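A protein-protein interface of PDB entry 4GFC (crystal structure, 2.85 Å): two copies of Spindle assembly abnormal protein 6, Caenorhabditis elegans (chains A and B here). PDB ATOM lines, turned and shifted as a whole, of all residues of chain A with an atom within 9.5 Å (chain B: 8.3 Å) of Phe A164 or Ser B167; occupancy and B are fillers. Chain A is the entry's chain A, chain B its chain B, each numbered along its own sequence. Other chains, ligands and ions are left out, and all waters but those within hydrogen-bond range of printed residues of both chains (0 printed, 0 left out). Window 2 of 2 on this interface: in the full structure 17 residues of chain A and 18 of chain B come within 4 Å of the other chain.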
ATOM      1  N   GLN A 157      -3.783  40.048 -13.720  1.00  0.00           N
ATOM      2  CA  GLN A 157      -3.154  39.655 -14.990  1.00  0.00           C
ATOM      3  C   GLN A 157      -1.609  39.591 -14.868  1.00  0.00           C
ATOM      4  O   GLN A 157      -0.935  39.089 -15.772  1.00  0.00           O
ATOM      5  CB  GLN A 157      -3.534  40.640 -16.104  1.00  0.00           C
ATOM      6  CG  GLN A 157      -4.957  40.513 -16.610  1.00  0.00           C
ATOM      7  CD  GLN A 157      -5.248  41.505 -17.708  1.00  0.00           C
ATOM      8  OE1 GLN A 157      -5.024  42.715 -17.575  1.00  0.00           O
ATOM      9  NE2 GLN A 157      -5.780  41.016 -18.815  1.00  0.00           N
ATOM     10  N   ALA A 158      -1.056  40.142 -13.765  1.00  0.00           N
ATOM     11  CA  ALA A 158       0.377  40.162 -13.472  1.00  0.00           C
ATOM     12  C   ALA A 158       0.818  38.817 -12.880  1.00  0.00           C
ATOM     13  O   ALA A 158       1.879  38.304 -13.251  1.00  0.00           O
ATOM     14  CB  ALA A 158       0.705  41.304 -12.518  1.00  0.00           C
ATOM     15  N   VAL A 159      -0.024  38.232 -11.990  1.00  0.00           N
ATOM     16  CA  VAL A 159       0.188  36.922 -11.349  1.00  0.00           C
ATOM     17  C   VAL A 159       0.121  35.825 -12.455  1.00  0.00           C
ATOM     18  O   VAL A 159       0.616  34.712 -12.263  1.00  0.00           O
ATOM     19  CB  VAL A 159      -0.809  36.676 -10.171  1.00  0.00           C
ATOM     20  CG1 VAL A 159      -0.500  35.379  -9.427  1.00  0.00           C
ATOM     21  CG2 VAL A 159      -0.800  37.847  -9.188  1.00  0.00           C
ATOM     22  N   LYS A 160      -0.432  36.191 -13.632  1.00  0.00           N
ATOM     23  CA  LYS A 160      -0.522  35.375 -14.840  1.00  0.00           C
ATOM     24  C   LYS A 160       0.899  35.171 -15.417  1.00  0.00           C
ATOM     25  O   LYS A 160       1.179  34.100 -15.946  1.00  0.00           O
ATOM     26  CB  LYS A 160      -1.469  36.051 -15.846  1.00  0.00           C
ATOM     27  CG  LYS A 160      -1.795  35.282 -17.112  1.00  0.00           C
ATOM     28  CD  LYS A 160      -2.820  36.057 -17.927  1.00  0.00           C
ATOM     29  CE  LYS A 160      -2.572  35.992 -19.413  1.00  0.00           C
ATOM     30  NZ  LYS A 160      -3.265  37.098 -20.128  1.00  0.00           N
ATOM     31  N   LEU A 161       1.806  36.169 -15.259  1.00  0.00           N
ATOM     32  CA  LEU A 161       3.208  36.076 -15.714  1.00  0.00           C
ATOM     33  C   LEU A 161       4.085  35.318 -14.681  1.00  0.00           C
ATOM     34  O   LEU A 161       5.098  34.726 -15.071  1.00  0.00           O
ATOM     35  CB  LEU A 161       3.797  37.488 -16.007  1.00  0.00           C
ATOM     36  CG  LEU A 161       5.310  37.630 -16.360  1.00  0.00           C
ATOM     37  CD1 LEU A 161       5.662  36.942 -17.677  1.00  0.00           C
ATOM     38  CD2 LEU A 161       5.722  39.085 -16.418  1.00  0.00           C
ATOM     39  N   SER A 162       3.696  35.342 -13.379  1.00  0.00           N
ATOM     40  CA  SER A 162       4.427  34.672 -12.293  1.00  0.00           C
ATOM     41  C   SER A 162       4.309  33.141 -12.407  1.00  0.00           C
ATOM     42  O   SER A 162       5.278  32.429 -12.109  1.00  0.00           O
ATOM     43  CB  SER A 162       3.943  35.150 -10.926  1.00  0.00           C
ATOM     44  OG  SER A 162       2.653  34.660 -10.600  1.00  0.00           O
ATOM     45  N   THR A 163       3.126  32.645 -12.850  1.00  0.00           N
ATOM     46  CA  THR A 163       2.859  31.218 -13.066  1.00  0.00           C
ATOM     47  C   THR A 163       3.466  30.795 -14.412  1.00  0.00           C
ATOM     48  O   THR A 163       4.008  29.695 -14.510  1.00  0.00           O
ATOM     49  CB  THR A 163       1.367  30.907 -12.965  1.00  0.00           C
ATOM     50  OG1 THR A 163       0.644  31.786 -13.827  1.00  0.00           O
ATOM     51  CG2 THR A 163       0.844  31.011 -11.534  1.00  0.00           C
ATOM     52  N   PHE A 164       3.472  31.708 -15.406  1.00  0.00           N
ATOM     53  CA  PHE A 164       4.081  31.504 -16.721  1.00  0.00           C
ATOM     54  C   PHE A 164       5.612  31.590 -16.634  1.00  0.00           C
ATOM     55  O   PHE A 164       6.326  31.106 -17.515  1.00  0.00           O
ATOM     56  CB  PHE A 164       3.548  32.548 -17.709  1.00  0.00           C
ATOM     57  CG  PHE A 164       2.404  32.069 -18.565  1.00  0.00           C
ATOM     58  CD1 PHE A 164       2.554  31.933 -19.936  1.00  0.00           C
ATOM     59  CD2 PHE A 164       1.175  31.751 -18.000  1.00  0.00           C
ATOM     60  CE1 PHE A 164       1.498  31.484 -20.728  1.00  0.00           C
ATOM     61  CE2 PHE A 164       0.115  31.308 -18.794  1.00  0.00           C
ATOM     62  CZ  PHE A 164       0.284  31.175 -20.153  1.00  0.00           C
ATOM     63  N   LYS A 166       8.082  29.021 -17.635  1.00  0.00           N
ATOM     64  CA  LYS A 166       9.413  29.263 -18.193  1.00  0.00           C
ATOM     65  C   LYS A 166       9.404  29.144 -19.733  1.00  0.00           C
ATOM     66  O   LYS A 166      10.465  28.957 -20.340  1.00  0.00           O
ATOM     67  CB  LYS A 166      10.440  28.292 -17.577  1.00  0.00           C
ATOM     68  CG  LYS A 166      10.800  28.598 -16.128  1.00  0.00           C
ATOM     69  CD  LYS A 166      11.740  27.547 -15.561  1.00  0.00           C
ATOM     70  CE  LYS A 166      12.039  27.778 -14.102  1.00  0.00           C
ATOM     71  NZ  LYS A 166      12.915  26.712 -13.547  1.00  0.00           N
ATOM     72  N   SER A 167       8.205  29.299 -20.355  1.00  0.00           N
ATOM     73  CA  SER A 167       7.910  29.217 -21.797  1.00  0.00           C
ATOM     74  C   SER A 167       8.347  27.852 -22.379  1.00  0.00           C
ATOM     75  O   SER A 167       9.460  27.712 -22.898  1.00  0.00           O
ATOM     76  CB  SER A 167       8.522  30.384 -22.574  1.00  0.00           C
ATOM     77  OG  SER A 167       9.940  30.353 -22.591  1.00  0.00           O
ATOM     78  N   ALA A 168       7.453  26.838 -22.240  1.00  0.00           N
ATOM     79  CA  ALA A 168       7.590  25.432 -22.670  1.00  0.00           C
ATOM     80  C   ALA A 168       8.831  24.732 -22.059  1.00  0.00           C
ATOM     81  O   ALA A 168       9.200  23.650 -22.520  1.00  0.00           O
ATOM     82  CB  ALA A 168       7.617  25.334 -24.195  1.00  0.00           C
ATOM     83  N   ASP A 169       9.425  25.327 -20.990  1.00  0.00           N
ATOM     84  CA  ASP A 169      10.624  24.876 -20.264  1.00  0.00           C
ATOM     85  C   ASP A 169      11.783  24.626 -21.251  1.00  0.00           C
ATOM     86  O   ASP A 169      12.319  23.513 -21.333  1.00  0.00           O
ATOM     87  CB  ASP A 169      10.332  23.641 -19.387  1.00  0.00           C
ATOM     88  CG  ASP A 169       9.696  23.969 -18.052  1.00  0.00           C
ATOM     89  OD1 ASP A 169      10.402  24.521 -17.177  1.00  0.00           O
ATOM     90  OD2 ASP A 169       8.508  23.636 -17.864  1.00  0.00           O
ATOM     91  N   GLU A 170      12.138  25.686 -22.018  1.00  0.00           N
ATOM     92  CA  GLU A 170      13.177  25.733 -23.063  1.00  0.00           C
ATOM     93  C   GLU A 170      12.837  24.752 -24.221  1.00  0.00           C
ATOM     94  O   GLU A 170      13.739  24.214 -24.870  1.00  0.00           O
ATOM     95  CB  GLU A 170      14.592  25.484 -22.486  1.00  0.00           C
ATOM     96  CG  GLU A 170      15.064  26.573 -21.534  1.00  0.00           C
ATOM     97  CD  GLU A 170      16.431  26.374 -20.906  1.00  0.00           C
ATOM     98  OE1 GLU A 170      16.704  25.264 -20.393  1.00  0.00           O
ATOM     99  OE2 GLU A 170      17.212  27.352 -20.877  1.00  0.00           O
ATOM    100  N   LYS B 160      -2.316  38.903 -24.303  1.00  0.00           N
ATOM    101  CA  LYS B 160      -1.440  37.924 -23.658  1.00  0.00           C
ATOM    102  C   LYS B 160      -2.211  36.595 -23.477  1.00  0.00           C
ATOM    103  O   LYS B 160      -1.605  35.534 -23.590  1.00  0.00           O
ATOM    104  CB  LYS B 160      -0.937  38.495 -22.319  1.00  0.00           C
ATOM    105  CG  LYS B 160       0.106  37.679 -21.570  1.00  0.00           C
ATOM    106  CD  LYS B 160       0.559  38.450 -20.338  1.00  0.00           C
ATOM    107  CE  LYS B 160       0.821  37.553 -19.158  1.00  0.00           C
ATOM    108  NZ  LYS B 160       0.743  38.297 -17.874  1.00  0.00           N
ATOM    109  N   LEU B 161      -3.546  36.650 -23.260  1.00  0.00           N
ATOM    110  CA  LEU B 161      -4.398  35.453 -23.129  1.00  0.00           C
ATOM    111  C   LEU B 161      -4.801  34.899 -24.519  1.00  0.00           C
ATOM    112  O   LEU B 161      -5.078  33.700 -24.629  1.00  0.00           O
ATOM    113  CB  LEU B 161      -5.659  35.756 -22.264  1.00  0.00           C
ATOM    114  CG  LEU B 161      -6.774  34.668 -22.124  1.00  0.00           C
ATOM    115  CD1 LEU B 161      -6.274  33.394 -21.425  1.00  0.00           C
ATOM    116  CD2 LEU B 161      -7.978  35.223 -21.392  1.00  0.00           C
ATOM    117  N   THR B 163      -2.830  34.794 -27.261  1.00  0.00           N
ATOM    118  CA  THR B 163      -1.672  34.032 -27.737  1.00  0.00           C
ATOM    119  C   THR B 163      -1.450  32.801 -26.847  1.00  0.00           C
ATOM    120  O   THR B 163      -1.222  31.696 -27.358  1.00  0.00           O
ATOM    121  CB  THR B 163      -0.409  34.909 -27.764  1.00  0.00           C
ATOM    122  OG1 THR B 163      -0.235  35.519 -26.485  1.00  0.00           O
ATOM    123  CG2 THR B 163      -0.445  35.965 -28.858  1.00  0.00           C
ATOM    124  N   PHE B 164      -1.460  33.024 -25.508  1.00  0.00           N
ATOM    125  CA  PHE B 164      -1.235  32.017 -24.471  1.00  0.00           C
ATOM    126  C   PHE B 164      -2.572  31.546 -23.856  1.00  0.00           C
ATOM    127  O   PHE B 164      -3.119  32.188 -22.948  1.00  0.00           O
ATOM    128  CB  PHE B 164      -0.293  32.567 -23.380  1.00  0.00           C
ATOM    129  CG  PHE B 164       1.032  33.131 -23.846  1.00  0.00           C
ATOM    130  CD1 PHE B 164       2.032  32.294 -24.331  1.00  0.00           C
ATOM    131  CD2 PHE B 164       1.301  34.490 -23.747  1.00  0.00           C
ATOM    132  CE1 PHE B 164       3.262  32.816 -24.751  1.00  0.00           C
ATOM    133  CE2 PHE B 164       2.530  35.012 -24.168  1.00  0.00           C
ATOM    134  CZ  PHE B 164       3.503  34.171 -24.663  1.00  0.00           C
ATOM    135  N   TYR B 165      -3.088  30.416 -24.376  1.00  0.00           N
ATOM    136  CA  TYR B 165      -4.352  29.786 -23.968  1.00  0.00           C
ATOM    137  C   TYR B 165      -4.252  28.246 -24.077  1.00  0.00           C
ATOM    138  O   TYR B 165      -4.848  27.535 -23.261  1.00  0.00           O
ATOM    139  CB  TYR B 165      -5.538  30.341 -24.800  1.00  0.00           C
ATOM    140  CG  TYR B 165      -5.536  29.975 -26.274  1.00  0.00           C
ATOM    141  CD1 TYR B 165      -6.434  29.039 -26.782  1.00  0.00           C
ATOM    142  CD2 TYR B 165      -4.658  30.587 -27.167  1.00  0.00           C
ATOM    143  CE1 TYR B 165      -6.444  28.706 -28.137  1.00  0.00           C
ATOM    144  CE2 TYR B 165      -4.649  30.251 -28.521  1.00  0.00           C
ATOM    145  CZ  TYR B 165      -5.546  29.311 -29.001  1.00  0.00           C
ATOM    146  OH  TYR B 165      -5.552  28.983 -30.334  1.00  0.00           O
ATOM    147  N   LYS B 166      -3.481  27.752 -25.079  1.00  0.00           N
ATOM    148  CA  LYS B 166      -3.212  26.337 -25.370  1.00  0.00           C
ATOM    149  C   LYS B 166      -1.849  25.895 -24.796  1.00  0.00           C
ATOM    150  O   LYS B 166      -1.438  24.751 -25.011  1.00  0.00           O
ATOM    151  CB  LYS B 166      -3.230  26.100 -26.893  1.00  0.00           C
ATOM    152  CG  LYS B 166      -4.577  25.686 -27.465  1.00  0.00           C
ATOM    153  CD  LYS B 166      -4.504  25.621 -28.987  1.00  0.00           C
ATOM    154  CE  LYS B 166      -5.833  25.329 -29.636  1.00  0.00           C
ATOM    155  NZ  LYS B 166      -5.736  25.345 -31.120  1.00  0.00           N
ATOM    156  N   SER B 167      -1.158  26.807 -24.072  1.00  0.00           N
ATOM    157  CA  SER B 167       0.173  26.627 -23.477  1.00  0.00           C
ATOM    158  C   SER B 167       0.269  25.412 -22.531  1.00  0.00           C
ATOM    159  O   SER B 167       1.100  24.532 -22.770  1.00  0.00           O
ATOM    160  CB  SER B 167       0.603  27.895 -22.739  1.00  0.00           C
ATOM    161  OG  SER B 167      -0.375  28.314 -21.802  1.00  0.00           O
ATOM    162  N   ALA B 168      -0.568  25.364 -21.475  1.00  0.00           N
ATOM    163  CA  ALA B 168      -0.583  24.286 -20.478  1.00  0.00           C
ATOM    164  C   ALA B 168      -1.023  22.945 -21.082  1.00  0.00           C
ATOM    165  O   ALA B 168      -0.523  21.893 -20.673  1.00  0.00           O
ATOM    166  CB  ALA B 168      -1.506  24.662 -19.327  1.00  0.00           C
ATOM    167  N   ASP B 169      -1.955  22.998 -22.053  1.00  0.00           N
ATOM    168  CA  ASP B 169      -2.543  21.846 -22.745  1.00  0.00           C
ATOM    169  C   ASP B 169      -1.517  21.154 -23.657  1.00  0.00           C
ATOM    170  O   ASP B 169      -1.406  19.930 -23.609  1.00  0.00           O
ATOM    171  CB  ASP B 169      -3.787  22.283 -23.547  1.00  0.00           C
ATOM    172  CG  ASP B 169      -4.703  23.233 -22.783  1.00  0.00           C
ATOM    173  OD1 ASP B 169      -5.597  22.742 -22.058  1.00  0.00           O
ATOM    174  OD2 ASP B 169      -4.497  24.464 -22.880  1.00  0.00           O
ATOM    175  N   GLU B 170      -0.756  21.933 -24.461  1.00  0.00           N
ATOM    176  CA  GLU B 170       0.278  21.424 -25.375  1.00  0.00           C
ATOM    177  C   GLU B 170       1.493  20.877 -24.616  1.00  0.00           C
ATOM    178  O   GLU B 170       2.210  20.027 -25.149  1.00  0.00           O
ATOM    179  CB  GLU B 170       0.728  22.516 -26.355  1.00  0.00           C
ATOM    180  CG  GLU B 170      -0.222  22.728 -27.519  1.00  0.00           C
ATOM    181  CD  GLU B 170       0.150  23.899 -28.405  1.00  0.00           C
ATOM    182  OE1 GLU B 170       0.772  23.668 -29.467  1.00  0.00           O
ATOM    183  OE2 GLU B 170      -0.170  25.053 -28.031  1.00  0.00           O
ATOM    184  N   LEU B 171       1.710  21.362 -23.374  1.00  0.00           N
ATOM    185  CA  LEU B 171       2.791  20.962 -22.467  1.00  0.00           C
ATOM    186  C   LEU B 171       2.654  19.482 -22.078  1.00  0.00           C
ATOM    187  O   LEU B 171       3.667  18.826 -21.839  1.00  0.00           O
ATOM    188  CB  LEU B 171       2.764  21.872 -21.218  1.00  0.00           C
ATOM    189  CG  LEU B 171       3.795  21.657 -20.097  1.00  0.00           C
ATOM    190  CD1 LEU B 171       5.191  22.116 -20.516  1.00  0.00           C
ATOM    191  CD2 LEU B 171       3.370  22.399 -18.842  1.00  0.00           C
ATOM    192  N   ALA B 172       1.408  18.959 -22.049  1.00  0.00           N
ATOM    193  CA  ALA B 172       1.096  17.568 -21.715  1.00  0.00           C
ATOM    194  C   ALA B 172       1.611  16.590 -22.780  1.00  0.00           C
ATOM    195  O   ALA B 172       2.243  15.594 -22.418  1.00  0.00           O
ATOM    196  CB  ALA B 172      -0.405  17.398 -21.536  1.00  0.00           C
ATOM    197  N   SER B 173       1.346  16.873 -24.082  1.00  0.00           N
ATOM    198  CA  SER B 173       1.763  16.030 -25.214  1.00  0.00           C
ATOM    199  C   SER B 173       3.289  15.922 -25.309  1.00  0.00           C
ATOM    200  O   SER B 173       3.798  14.832 -25.564  1.00  0.00           O
ATOM    201  CB  SER B 173       1.194  16.556 -26.530  1.00  0.00           C
ATOM    202  OG  SER B 173       1.704  17.836 -26.869  1.00  0.00           O
ATOM    203  N   LEU B 174       4.008  17.040 -25.071  1.00  0.00           N
ATOM    204  CA  LEU B 174       5.471  17.093 -25.116  1.00  0.00           C
ATOM    205  C   LEU B 174       6.105  16.455 -23.864  1.00  0.00           C
ATOM    206  O   LEU B 174       7.132  15.788 -24.003  1.00  0.00           O
ATOM    207  CB  LEU B 174       5.989  18.538 -25.307  1.00  0.00           C
ATOM    208  CG  LEU B 174       5.630  19.266 -26.624  1.00  0.00           C
ATOM    209  CD1 LEU B 174       6.010  20.731 -26.552  1.00  0.00           C
ATOM    210  CD2 LEU B 174       6.311  18.631 -27.833  1.00  0.00           C
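The backbone carbonyl oxygen (O) of Gln A157 sits at hydrogen-bond distance from the side-chain amino group (NZ) of Lys B160 (2.8 Å). The side-chain amino group (NZ) of Lys A160 sits close to the backbone NH (N) of Leu B161 (3.2 Å).
The backbone carbonyl oxygen (O) of Lys B160 is in hydrogen-bond range of the side-chain hydroxyl (OG1) of Thr B163 (3.2 Å). The backbone carbonyl oxygen of Lys A160 is in hydrogen-bond range of the side-chain hydroxyl of Thr A163 (3.2 Å).
Lys B160 touches Lys A160 (CB to NZ, 3.5 Å). N of Leu A161 touches NZ of Lys B160 (3.5 Å). CB of Phe B164 touches CE1 of Phe A164, 3.4 Å away. Phe A164 touches Ser B167.
Of chain A, only Phe A164 (3.4 Å) comes within 4 Å of Ser B167. Printed residues of chain A within 4 Å of Lys B160: Gln A157 (2.8 Å), Lys A160 (3.5 Å) and Leu A161 (3.5 Å). Of the printed residues of chain B, Leu A161 touches Lys B160. Printed residues of chain A within 4 Å of Phe B164: Phe A164. Asp A169 touches none of the printed residues of chain B. Asp B169 touches none of the printed residues of chain A. The nearest residue of chain B that does not touch Phe A164 is Tyr B165 (5.5 Å). The nearest residue of chain A that does not touch Ser B167 is Ala A168 (6.6 Å).
Printed residues of chain B that touch a printed residue of chain A: Lys B160, Leu B161, Phe B164 and Ser B167. Hydrophobic or aromatic side chains of chain B that line the printed part of chain A: Leu B161 and Phe B164. Printed residues of chain A that touch a printed residue of chain B: Gln A157, Lys A160, Leu A161 and Phe A164. Hydrophobic or aromatic side chains of chain A within 4 Å of the printed part of chain B: Leu A161 and Phe A164. Along chain A the printed residues that touch a printed residue of chain B span positions 157 to 164. Among the printed residues, 6 pairs touch across the chains. Among the printed residues, no Asp or Glu carboxylate lies within 4 Å of a Lys or Arg side-chain nitrogen of the other chain.
Lys A160 touches its own counterpart, Lys B160. Lys A160 touches Leu B161, and with the chains exchanged Leu A161 touches Lys B160. Phe B164 touches its own counterpart, Phe A164. Phe A164 touches Ser B167, but with the chains exchanged Ser A167 does not touch Phe B164 (6.2 Å). Positions printed for both chains: 160, 161, 163, 164, 166, 167, 168, 169 and 170. Of the 6 pairs that touch across the chains among the printed residues, 4 have their exchanged pair printed and touching as well.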
